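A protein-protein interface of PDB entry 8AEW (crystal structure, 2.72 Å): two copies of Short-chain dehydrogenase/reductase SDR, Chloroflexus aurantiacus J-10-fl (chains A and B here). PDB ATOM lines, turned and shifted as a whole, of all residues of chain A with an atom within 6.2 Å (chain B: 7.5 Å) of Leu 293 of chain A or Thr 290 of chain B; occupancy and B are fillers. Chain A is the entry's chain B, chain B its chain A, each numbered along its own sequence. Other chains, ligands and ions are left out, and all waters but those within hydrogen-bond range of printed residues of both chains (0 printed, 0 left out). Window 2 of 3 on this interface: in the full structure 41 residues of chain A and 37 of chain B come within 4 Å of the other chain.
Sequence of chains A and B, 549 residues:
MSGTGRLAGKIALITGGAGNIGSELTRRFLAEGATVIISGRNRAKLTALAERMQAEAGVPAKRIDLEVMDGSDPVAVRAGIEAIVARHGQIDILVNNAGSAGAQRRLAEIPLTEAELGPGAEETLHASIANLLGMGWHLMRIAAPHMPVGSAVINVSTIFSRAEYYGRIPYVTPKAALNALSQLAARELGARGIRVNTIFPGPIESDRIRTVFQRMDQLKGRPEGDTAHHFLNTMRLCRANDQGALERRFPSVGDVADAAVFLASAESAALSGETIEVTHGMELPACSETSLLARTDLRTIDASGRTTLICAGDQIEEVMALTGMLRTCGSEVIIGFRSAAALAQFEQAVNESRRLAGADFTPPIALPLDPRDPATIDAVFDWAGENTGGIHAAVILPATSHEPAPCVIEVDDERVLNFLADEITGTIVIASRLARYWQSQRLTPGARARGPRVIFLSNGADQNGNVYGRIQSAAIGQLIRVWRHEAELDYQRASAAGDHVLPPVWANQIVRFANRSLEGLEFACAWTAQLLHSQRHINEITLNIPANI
OG1 of Thr 290 of chain A is in hydrogen-bond range of OG1 of Thr 290 of chain B, 3.0 Å away.
The side-chain hydroxyl (OG1) of Thr 290 of chain A sits at hydrogen-bond distance from the backbone NH (N) of Ser 291 of chain B (3.0 Å).
N of Ser 291 of chain A is in hydrogen-bond range of OG1 of Thr 290 of chain B, 2.9 Å away.
The side-chain carboxylate (OE2) of Glu 540 of chain B sits at hydrogen-bond distance from the side-chain hydroxyl (OG) of Ser 291 of chain A (2.7 Å).
The backbone carbonyl oxygen (O) of Thr 290 of chain A sits at hydrogen-bond distance from the backbone NH (N) of Asn 544 of chain A, at 2.9 Å.
The backbone carbonyl oxygen (O) of Ala 294 of chain A lies within hydrogen-bond range of the indole nitrogen (NE1) of Trp 527 of chain A, at 3.3 Å.
The backbone NH (N) of Thr 290 of chain B sits at hydrogen-bond distance from the backbone carbonyl oxygen (O) of Thr 542 of chain B.
The backbone carbonyl oxygen (O) of Thr 290 of chain B sits at hydrogen-bond distance from the backbone NH (N) of Asn 544 of chain B (2.9 Å).
The backbone carbonyl oxygen (O) of Ala 294 of chain B is in hydrogen-bond range of the indole nitrogen (NE1) of Trp 527 of chain B (3.4 Å).
Among the printed residues, pairs that only touch across the chains: Ala 294 of chain A with Ala 294 of chain B (3.5 Å) and Leu 293 of chain A with Thr 290 of chain B (3.95 Å).
Of chain B, only Thr 290 (3.95 Å) comes within 4 Å of Leu 293 of chain A.
Printed residues of chain A within 4 Å of Ser 291 of chain B: Thr 290.
Of the printed residues of chain B, Ala 294 of chain A touches Ala 294 (3.5 Å).
Of the printed residues of chain B, Thr 290 of chain A touches Thr 290 (3.0 Å) and Ser 291 (3.0 Å).
The nearest residue of chain B that does not touch Leu 293 of chain A is Ile 538 of chain B (4.1 Å).
The nearest printed residue of chain B that does not touch Ser 291 of chain A is Ser 291 of chain B (4.6 Å).
Of the 21 printed residues of chain B, 4 touch a printed residue of chain A.
Hydrophobic or aromatic side chains of chain B within 4 Å of the printed part of chain A: Ala 294.
Printed residues of chain A that touch a printed residue of chain B: Thr 290, Ser 291, Leu 293 and Ala 294.
Along chain A the printed residues that touch a printed residue of chain B span positions 290 to 294.
Among the printed residues, 6 pairs touch across the chains.
Among the printed residues, no Asp or Glu carboxylate lies within 4 Å of a Lys or Arg side-chain nitrogen of the other chain.
Thr 290 of chain A touches its own counterpart, Thr 290 of chain B.
Thr 290 of chain A touches Ser 291 of chain B, and with the chains exchanged Ser 291 of chain A touches Thr 290 of chain B.
Leu 293 of chain A touches Thr 290 of chain B, but with the chains exchanged Thr 290 of chain A does not touch Leu 293 of chain B (4.3 Å).
Ala 294 of chain B touches its own counterpart, Ala 294 of chain A.
Of the 6 pairs that touch across the chains among the printed residues, 4 have their exchanged pair printed and touching as well.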
ATOM      1  N   GLU A 289     -23.399   9.259 -28.338  1.00  0.00           N
ATOM      2  CA  GLU A 289     -22.951   9.828 -27.083  1.00  0.00           C
ATOM      3  C   GLU A 289     -23.613  11.182 -26.868  1.00  0.00           C
ATOM      4  O   GLU A 289     -24.105  11.812 -27.805  1.00  0.00           O
ATOM      5  CB  GLU A 289     -21.423   9.952 -27.040  1.00  0.00           C
ATOM      6  CG  GLU A 289     -20.720   8.611 -27.149  1.00  0.00           C
ATOM      7  CD  GLU A 289     -19.202   8.669 -26.940  1.00  0.00           C
ATOM      8  OE1 GLU A 289     -18.650   9.769 -26.701  1.00  0.00           O
ATOM      9  OE2 GLU A 289     -18.556   7.593 -27.039  1.00  0.00           O
ATOM     10  N   THR A 290     -23.629  11.622 -25.612  1.00  0.00           N
ATOM     11  CA  THR A 290     -24.168  12.926 -25.271  1.00  0.00           C
ATOM     12  C   THR A 290     -23.515  13.401 -23.979  1.00  0.00           C
ATOM     13  O   THR A 290     -23.045  12.599 -23.165  1.00  0.00           O
ATOM     14  CB  THR A 290     -25.700  12.882 -25.131  1.00  0.00           C
ATOM     15  OG1 THR A 290     -26.218  14.213 -25.017  1.00  0.00           O
ATOM     16  CG2 THR A 290     -26.110  12.102 -23.903  1.00  0.00           C
ATOM     17  N   SER A 291     -23.462  14.717 -23.818  1.00  0.00           N
ATOM     18  CA  SER A 291     -22.921  15.339 -22.622  1.00  0.00           C
ATOM     19  C   SER A 291     -24.047  15.648 -21.652  1.00  0.00           C
ATOM     20  O   SER A 291     -25.113  16.132 -22.054  1.00  0.00           O
ATOM     21  CB  SER A 291     -22.146  16.617 -22.964  1.00  0.00           C
ATOM     22  OG  SER A 291     -20.975  16.326 -23.729  1.00  0.00           O
ATOM     23  N   LEU A 292     -23.805  15.351 -20.372  1.00  0.00           N
ATOM     24  CA  LEU A 292     -24.659  15.817 -19.284  1.00  0.00           C
ATOM     25  C   LEU A 292     -24.309  17.279 -19.081  1.00  0.00           C
ATOM     26  O   LEU A 292     -23.242  17.599 -18.549  1.00  0.00           O
ATOM     27  CB  LEU A 292     -24.435  15.011 -18.004  1.00  0.00           C
ATOM     28  CG  LEU A 292     -24.637  13.489 -18.054  1.00  0.00           C
ATOM     29  CD1 LEU A 292     -24.132  12.852 -16.779  1.00  0.00           C
ATOM     30  CD2 LEU A 292     -26.071  13.062 -18.355  1.00  0.00           C
ATOM     31  N   LEU A 293     -25.194  18.160 -19.538  1.00  0.00           N
ATOM     32  CA  LEU A 293     -24.949  19.591 -19.515  1.00  0.00           C
ATOM     33  C   LEU A 293     -25.714  20.311 -18.413  1.00  0.00           C
ATOM     34  O   LEU A 293     -25.289  21.391 -17.986  1.00  0.00           O
ATOM     35  CB  LEU A 293     -25.352  20.193 -20.865  1.00  0.00           C
ATOM     36  CG  LEU A 293     -24.593  19.610 -22.047  1.00  0.00           C
ATOM     37  CD1 LEU A 293     -25.174  20.117 -23.336  1.00  0.00           C
ATOM     38  CD2 LEU A 293     -23.118  19.954 -21.949  1.00  0.00           C
ATOM     39  N   ALA A 294     -26.807  19.731 -17.930  1.00  0.00           N
ATOM     40  CA  ALA A 294     -27.675  20.396 -16.974  1.00  0.00           C
ATOM     41  C   ALA A 294     -27.257  20.084 -15.542  1.00  0.00           C
ATOM     42  O   ALA A 294     -26.532  19.121 -15.282  1.00  0.00           O
ATOM     43  CB  ALA A 294     -29.123  19.965 -17.191  1.00  0.00           C
ATOM     44  N   ARG A 295     -27.732  20.919 -14.609  1.00  0.00           N
ATOM     45  CA  ARG A 295     -27.644  20.594 -13.187  1.00  0.00           C
ATOM     46  C   ARG A 295     -28.660  19.515 -12.838  1.00  0.00           C
ATOM     47  O   ARG A 295     -29.787  19.514 -13.337  1.00  0.00           O
ATOM     48  CB  ARG A 295     -27.883  21.836 -12.328  1.00  0.00           C
ATOM     49  N   PHE A 523     -20.820  16.279  -9.269  1.00  0.00           N
ATOM     50  CA  PHE A 523     -21.777  16.367 -10.363  1.00  0.00           C
ATOM     51  C   PHE A 523     -22.062  14.996 -10.958  1.00  0.00           C
ATOM     52  O   PHE A 523     -23.221  14.654 -11.228  1.00  0.00           O
ATOM     53  CB  PHE A 523     -21.235  17.331 -11.417  1.00  0.00           C
ATOM     54  CG  PHE A 523     -22.113  17.478 -12.623  1.00  0.00           C
ATOM     55  CD1 PHE A 523     -23.290  18.196 -12.559  1.00  0.00           C
ATOM     56  CD2 PHE A 523     -21.749  16.911 -13.833  1.00  0.00           C
ATOM     57  CE1 PHE A 523     -24.090  18.325 -13.678  1.00  0.00           C
ATOM     58  CE2 PHE A 523     -22.546  17.044 -14.954  1.00  0.00           C
ATOM     59  CZ  PHE A 523     -23.716  17.744 -14.875  1.00  0.00           C
ATOM     60  N   TRP A 527     -25.675  12.735 -10.830  1.00  0.00           N
ATOM     61  CA  TRP A 527     -26.416  12.178 -11.958  1.00  0.00           C
ATOM     62  C   TRP A 527     -26.602  10.671 -11.824  1.00  0.00           C
ATOM     63  O   TRP A 527     -27.636  10.132 -12.233  1.00  0.00           O
ATOM     64  CB  TRP A 527     -25.741  12.543 -13.282  1.00  0.00           C
ATOM     65  CG  TRP A 527     -26.201  13.844 -13.775  1.00  0.00           C
ATOM     66  CD1 TRP A 527     -25.553  15.038 -13.696  1.00  0.00           C
ATOM     67  CD2 TRP A 527     -27.468  14.106 -14.381  1.00  0.00           C
ATOM     68  NE1 TRP A 527     -26.332  16.033 -14.242  1.00  0.00           N
ATOM     69  CE2 TRP A 527     -27.517  15.486 -14.664  1.00  0.00           C
ATOM     70  CE3 TRP A 527     -28.566  13.305 -14.717  1.00  0.00           C
ATOM     71  CZ2 TRP A 527     -28.624  16.086 -15.268  1.00  0.00           C
ATOM     72  CZ3 TRP A 527     -29.657  13.894 -15.318  1.00  0.00           C
ATOM     73  CH2 TRP A 527     -29.680  15.274 -15.591  1.00  0.00           C
ATOM     74  N   ASN A 544     -21.333  11.855 -20.919  1.00  0.00           N
ATOM     75  CA  ASN A 544     -20.071  12.554 -20.714  1.00  0.00           C
ATOM     76  C   ASN A 544     -20.247  13.765 -19.812  1.00  0.00           C
ATOM     77  O   ASN A 544     -21.211  14.527 -19.954  1.00  0.00           O
ATOM     78  CB  ASN A 544     -19.501  13.006 -22.060  1.00  0.00           C
ATOM     79  CG  ASN A 544     -18.837  11.888 -22.805  1.00  0.00           C
ATOM     80  OD1 ASN A 544     -17.950  11.224 -22.263  1.00  0.00           O
ATOM     81  ND2 ASN A 544     -19.296  11.625 -24.030  1.00  0.00           N
ATOM     82  N   PRO A 546     -18.551  17.349 -18.760  1.00  0.00           N
ATOM     83  CA  PRO A 546     -17.563  18.260 -19.352  1.00  0.00           C
ATOM     84  C   PRO A 546     -16.611  18.845 -18.327  1.00  0.00           C
ATOM     85  O   PRO A 546     -16.636  18.432 -17.167  1.00  0.00           O
ATOM     86  CB  PRO A 546     -18.442  19.337 -19.986  1.00  0.00           C
ATOM     87  CG  PRO A 546     -19.703  19.302 -19.191  1.00  0.00           C
ATOM     88  CD  PRO A 546     -19.915  17.907 -18.786  1.00  0.00           C
ATOM     89  N   CYS B 287     -16.098  13.833 -33.479  1.00  0.00           N
ATOM     90  CA  CYS B 287     -17.467  14.192 -33.110  1.00  0.00           C
ATOM     91  C   CYS B 287     -17.455  15.363 -32.128  1.00  0.00           C
ATOM     92  O   CYS B 287     -16.742  15.323 -31.123  1.00  0.00           O
ATOM     93  CB  CYS B 287     -18.248  12.995 -32.552  1.00  0.00           C
ATOM     94  SG  CYS B 287     -19.223  12.002 -33.801  1.00  0.00           S
ATOM     95  N   SER B 288     -18.139  16.452 -32.509  1.00  0.00           N
ATOM     96  CA  SER B 288     -18.414  17.630 -31.683  1.00  0.00           C
ATOM     97  C   SER B 288     -19.922  17.828 -31.469  1.00  0.00           C
ATOM     98  O   SER B 288     -20.448  18.933 -31.665  1.00  0.00           O
ATOM     99  CB  SER B 288     -17.789  18.882 -32.322  1.00  0.00           C
ATOM    100  OG  SER B 288     -18.048  20.083 -31.600  1.00  0.00           O
ATOM    101  N   GLU B 289     -20.632  16.772 -31.061  1.00  0.00           N
ATOM    102  CA  GLU B 289     -22.081  16.818 -30.925  1.00  0.00           C
ATOM    103  C   GLU B 289     -22.545  16.395 -29.538  1.00  0.00           C
ATOM    104  O   GLU B 289     -21.789  15.815 -28.752  1.00  0.00           O
ATOM    105  CB  GLU B 289     -22.773  15.955 -31.973  1.00  0.00           C
ATOM    106  CG  GLU B 289     -23.028  16.674 -33.269  1.00  0.00           C
ATOM    107  CD  GLU B 289     -23.696  15.790 -34.312  1.00  0.00           C
ATOM    108  OE1 GLU B 289     -23.591  14.545 -34.224  1.00  0.00           O
ATOM    109  OE2 GLU B 289     -24.402  16.341 -35.185  1.00  0.00           O
ATOM    110  N   THR B 290     -23.784  16.793 -29.230  1.00  0.00           N
ATOM    111  CA  THR B 290     -24.489  16.420 -28.012  1.00  0.00           C
ATOM    112  C   THR B 290     -25.982  16.635 -28.234  1.00  0.00           C
ATOM    113  O   THR B 290     -26.387  17.426 -29.082  1.00  0.00           O
ATOM    114  CB  THR B 290     -23.996  17.225 -26.811  1.00  0.00           C
ATOM    115  OG1 THR B 290     -24.558  16.679 -25.614  1.00  0.00           O
ATOM    116  CG2 THR B 290     -24.436  18.664 -26.936  1.00  0.00           C
ATOM    117  N   SER B 291     -26.801  15.936 -27.447  1.00  0.00           N
ATOM    118  CA  SER B 291     -28.250  16.136 -27.474  1.00  0.00           C
ATOM    119  C   SER B 291     -28.643  17.202 -26.467  1.00  0.00           C
ATOM    120  O   SER B 291     -28.083  17.278 -25.369  1.00  0.00           O
ATOM    121  CB  SER B 291     -29.037  14.866 -27.139  1.00  0.00           C
ATOM    122  OG  SER B 291     -29.108  13.926 -28.186  1.00  0.00           O
ATOM    123  N   LEU B 292     -29.563  18.064 -26.872  1.00  0.00           N
ATOM    124  CA  LEU B 292     -30.249  18.914 -25.906  1.00  0.00           C
ATOM    125  C   LEU B 292     -31.319  18.051 -25.248  1.00  0.00           C
ATOM    126  O   LEU B 292     -32.373  17.786 -25.832  1.00  0.00           O
ATOM    127  CB  LEU B 292     -30.831  20.148 -26.583  1.00  0.00           C
ATOM    128  CG  LEU B 292     -29.692  21.062 -26.995  1.00  0.00           C
ATOM    129  CD1 LEU B 292     -30.207  22.241 -27.780  1.00  0.00           C
ATOM    130  CD2 LEU B 292     -28.940  21.508 -25.744  1.00  0.00           C
ATOM    131  N   LEU B 293     -31.038  17.581 -24.035  1.00  0.00           N
ATOM    132  CA  LEU B 293     -31.950  16.683 -23.353  1.00  0.00           C
ATOM    133  C   LEU B 293     -32.666  17.320 -22.178  1.00  0.00           C
ATOM    134  O   LEU B 293     -33.680  16.774 -21.731  1.00  0.00           O
ATOM    135  CB  LEU B 293     -31.228  15.413 -22.873  1.00  0.00           C
ATOM    136  CG  LEU B 293     -30.707  14.392 -23.895  1.00  0.00           C
ATOM    137  CD1 LEU B 293     -30.175  13.190 -23.146  1.00  0.00           C
ATOM    138  CD2 LEU B 293     -31.756  13.964 -24.916  1.00  0.00           C
ATOM    139  N   ALA B 294     -32.156  18.435 -21.661  1.00  0.00           N
ATOM    140  CA  ALA B 294     -32.637  19.040 -20.427  1.00  0.00           C
ATOM    141  C   ALA B 294     -33.774  20.031 -20.662  1.00  0.00           C
ATOM    142  O   ALA B 294     -34.009  20.515 -21.766  1.00  0.00           O
ATOM    143  CB  ALA B 294     -31.496  19.747 -19.703  1.00  0.00           C
ATOM    144  N   GLN B 509     -24.844  25.634 -33.246  1.00  0.00           N
ATOM    145  CA  GLN B 509     -26.025  25.417 -34.071  1.00  0.00           C
ATOM    146  C   GLN B 509     -26.914  24.361 -33.435  1.00  0.00           C
ATOM    147  O   GLN B 509     -26.437  23.406 -32.809  1.00  0.00           O
ATOM    148  CB  GLN B 509     -25.721  24.986 -35.524  1.00  0.00           C
ATOM    149  CG  GLN B 509     -24.919  23.724 -35.660  1.00  0.00           C
ATOM    150  CD  GLN B 509     -24.969  23.139 -37.059  1.00  0.00           C
ATOM    151  OE1 GLN B 509     -25.834  23.496 -37.865  1.00  0.00           O
ATOM    152  NE2 GLN B 509     -24.016  22.257 -37.370  1.00  0.00           N
ATOM    153  N   TRP B 527     -34.268  27.176 -26.158  1.00  0.00           N
ATOM    154  CA  TRP B 527     -32.823  27.055 -25.985  1.00  0.00           C
ATOM    155  C   TRP B 527     -32.086  28.085 -26.823  1.00  0.00           C
ATOM    156  O   TRP B 527     -31.062  28.623 -26.389  1.00  0.00           O
ATOM    157  CB  TRP B 527     -32.330  25.653 -26.344  1.00  0.00           C
ATOM    158  CG  TRP B 527     -32.404  24.611 -25.247  1.00  0.00           C
ATOM    159  CD1 TRP B 527     -33.320  23.611 -25.121  1.00  0.00           C
ATOM    160  CD2 TRP B 527     -31.491  24.463 -24.149  1.00  0.00           C
ATOM    161  NE1 TRP B 527     -33.039  22.857 -24.006  1.00  0.00           N
ATOM    162  CE2 TRP B 527     -31.921  23.359 -23.394  1.00  0.00           C
ATOM    163  CE3 TRP B 527     -30.355  25.163 -23.732  1.00  0.00           C
ATOM    164  CZ2 TRP B 527     -31.257  22.933 -22.255  1.00  0.00           C
ATOM    165  CZ3 TRP B 527     -29.701  24.740 -22.595  1.00  0.00           C
ATOM    166  CH2 TRP B 527     -30.151  23.634 -21.873  1.00  0.00           C
ATOM    167  N   ARG B 536     -23.192  31.306 -18.954  1.00  0.00           N
ATOM    168  CA  ARG B 536     -22.426  30.133 -19.348  1.00  0.00           C
ATOM    169  C   ARG B 536     -22.540  29.922 -20.860  1.00  0.00           C
ATOM    170  O   ARG B 536     -23.208  30.681 -21.564  1.00  0.00           O
ATOM    171  CB  ARG B 536     -22.913  28.911 -18.579  1.00  0.00           C
ATOM    172  CG  ARG B 536     -22.732  29.057 -17.099  1.00  0.00           C
ATOM    173  CD  ARG B 536     -23.028  27.763 -16.372  1.00  0.00           C
ATOM    174  NE  ARG B 536     -22.907  27.965 -14.938  1.00  0.00           N
ATOM    175  CZ  ARG B 536     -21.747  28.025 -14.299  1.00  0.00           C
ATOM    176  NH1 ARG B 536     -20.597  27.912 -14.950  1.00  0.00           N
ATOM    177  NH2 ARG B 536     -21.737  28.233 -12.983  1.00  0.00           N
ATOM    178  N   HIS B 537     -21.900  28.866 -21.367  1.00  0.00           N
ATOM    179  CA  HIS B 537     -21.973  28.503 -22.784  1.00  0.00           C
ATOM    180  C   HIS B 537     -21.888  26.991 -22.904  1.00  0.00           C
ATOM    181  O   HIS B 537     -21.520  26.301 -21.949  1.00  0.00           O
ATOM    182  CB  HIS B 537     -20.850  29.114 -23.631  1.00  0.00           C
ATOM    183  CG  HIS B 537     -19.523  28.455 -23.417  1.00  0.00           C
ATOM    184  ND1 HIS B 537     -18.678  28.792 -22.382  1.00  0.00           N
ATOM    185  CD2 HIS B 537     -18.910  27.447 -24.086  1.00  0.00           C
ATOM    186  CE1 HIS B 537     -17.594  28.037 -22.430  1.00  0.00           C
ATOM    187  NE2 HIS B 537     -17.710  27.211 -23.455  1.00  0.00           N
ATOM    188  N   ILE B 538     -22.261  26.479 -24.082  1.00  0.00           N
ATOM    189  CA  ILE B 538     -22.083  25.075 -24.434  1.00  0.00           C
ATOM    190  C   ILE B 538     -20.878  24.938 -25.361  1.00  0.00           C
ATOM    191  O   ILE B 538     -20.646  25.804 -26.219  1.00  0.00           O
ATOM    192  CB  ILE B 538     -23.356  24.499 -25.074  1.00  0.00           C
ATOM    193  CG1 ILE B 538     -24.468  24.415 -24.031  1.00  0.00           C
ATOM    194  CG2 ILE B 538     -23.074  23.136 -25.710  1.00  0.00           C
ATOM    195  CD1 ILE B 538     -25.811  23.988 -24.580  1.00  0.00           C
ATOM    196  N   ASN B 539     -20.076  23.867 -25.168  1.00  0.00           N
ATOM    197  CA  ASN B 539     -18.854  23.678 -25.959  1.00  0.00           C
ATOM    198  C   ASN B 539     -19.124  23.036 -27.314  1.00  0.00           C
ATOM    199  O   ASN B 539     -18.657  23.527 -28.343  1.00  0.00           O
ATOM    200  CB  ASN B 539     -17.840  22.820 -25.206  1.00  0.00           C
ATOM    201  CG  ASN B 539     -17.154  23.572 -24.095  1.00  0.00           C
ATOM    202  OD1 ASN B 539     -16.792  24.746 -24.246  1.00  0.00           O
ATOM    203  ND2 ASN B 539     -16.958  22.894 -22.961  1.00  0.00           N
ATOM    204  N   GLU B 540     -19.850  21.922 -27.325  1.00  0.00           N
ATOM    205  CA  GLU B 540     -20.256  21.267 -28.559  1.00  0.00           C
ATOM    206  C   GLU B 540     -20.726  22.276 -29.600  1.00  0.00           C
ATOM    207  O   GLU B 540     -21.355  23.286 -29.265  1.00  0.00           O
ATOM    208  CB  GLU B 540     -21.360  20.250 -28.262  1.00  0.00           C
ATOM    209  CG  GLU B 540     -20.868  18.914 -27.685  1.00  0.00           C
ATOM    210  CD  GLU B 540     -20.499  18.957 -26.214  1.00  0.00           C
ATOM    211  OE1 GLU B 540     -20.618  20.027 -25.585  1.00  0.00           O
ATOM    212  OE2 GLU B 540     -20.084  17.907 -25.685  1.00  0.00           O
ATOM    213  N   ILE B 541     -20.349  22.024 -30.863  1.00  0.00           N
ATOM    214  CA  ILE B 541     -20.739  22.902 -31.963  1.00  0.00           C
ATOM    215  C   ILE B 541     -22.188  22.637 -32.390  1.00  0.00           C
ATOM    216  O   ILE B 541     -22.986  23.569 -32.568  1.00  0.00           O
ATOM    217  CB  ILE B 541     -19.736  22.746 -33.131  1.00  0.00           C
ATOM    218  CG1 ILE B 541     -18.339  23.177 -32.656  1.00  0.00           C
ATOM    219  CG2 ILE B 541     -20.184  23.547 -34.373  1.00  0.00           C
ATOM    220  CD1 ILE B 541     -17.224  22.856 -33.582  1.00  0.00           C
ATOM    221  N   THR B 542     -22.564  21.371 -32.536  1.00  0.00           N
ATOM    222  CA  THR B 542     -23.897  21.006 -32.996  1.00  0.00           C
ATOM    223  C   THR B 542     -24.728  20.435 -31.841  1.00  0.00           C
ATOM    224  O   THR B 542     -24.289  19.527 -31.119  1.00  0.00           O
ATOM    225  CB  THR B 542     -23.790  20.033 -34.174  1.00  0.00           C
ATOM    226  OG1 THR B 542     -23.226  20.734 -35.286  1.00  0.00           O
ATOM    227  CG2 THR B 542     -25.127  19.479 -34.586  1.00  0.00           C
ATOM    228  N   LEU B 543     -25.929  20.980 -31.672  1.00  0.00           N
ATOM    229  CA  LEU B 543     -26.810  20.639 -30.562  1.00  0.00           C
ATOM    230  C   LEU B 543     -28.067  20.032 -31.166  1.00  0.00           C
ATOM    231  O   LEU B 543     -28.781  20.688 -31.933  1.00  0.00           O
ATOM    232  CB  LEU B 543     -27.133  21.880 -29.724  1.00  0.00           C
ATOM    233  CG  LEU B 543     -25.885  22.646 -29.270  1.00  0.00           C
ATOM    234  CD1 LEU B 543     -26.202  23.956 -28.561  1.00  0.00           C
ATOM    235  CD2 LEU B 543     -25.017  21.776 -28.423  1.00  0.00           C
ATOM    236  N   ASN B 544     -28.340  18.785 -30.820  1.00  0.00           N
ATOM    237  CA  ASN B 544     -29.383  18.006 -31.466  1.00  0.00           C
ATOM    238  C   ASN B 544     -30.573  17.877 -30.527  1.00  0.00           C
ATOM    239  O   ASN B 544     -30.400  17.601 -29.336  1.00  0.00           O
ATOM    240  CB  ASN B 544     -28.815  16.642 -31.847  1.00  0.00           C
ATOM    241  CG  ASN B 544     -27.871  16.722 -33.038  1.00  0.00           C
ATOM    242  OD1 ASN B 544     -28.254  17.168 -34.111  1.00  0.00           O
ATOM    243  ND2 ASN B 544     -26.613  16.371 -32.821  1.00  0.00           N
ATOM    244  N   ILE B 545     -31.771  18.084 -31.057  1.00  0.00           N
ATOM    245  CA  ILE B 545     -32.998  17.997 -30.276  1.00  0.00           C
ATOM    246  C   ILE B 545     -33.664  16.660 -30.599  1.00  0.00           C
ATOM    247  O   ILE B 545     -33.874  16.356 -31.780  1.00  0.00           O
ATOM    248  CB  ILE B 545     -33.914  19.202 -30.548  1.00  0.00           C
ATOM    249  CG1 ILE B 545     -34.556  19.171 -31.923  1.00  0.00           C
ATOM    250  CG2 ILE B 545     -33.088  20.482 -30.545  1.00  0.00           C
ATOM    251  CD1 ILE B 545     -35.644  20.198 -32.099  1.00  0.00           C
ATOM    252  N   PRO B 546     -33.960  15.823 -29.615  1.00  0.00           N
ATOM    253  CA  PRO B 546     -34.391  14.457 -29.942  1.00  0.00           C
ATOM    254  C   PRO B 546     -35.851  14.364 -30.343  1.00  0.00           C
ATOM    255  O   PRO B 546     -36.491  15.395 -30.543  1.00  0.00           O
ATOM    256  CB  PRO B 546     -34.094  13.684 -28.655  1.00  0.00           C
ATOM    257  CG  PRO B 546     -34.086  14.717 -27.588  1.00  0.00           C
ATOM    258  CD  PRO B 546     -33.569  15.964 -28.206  1.00  0.00           C
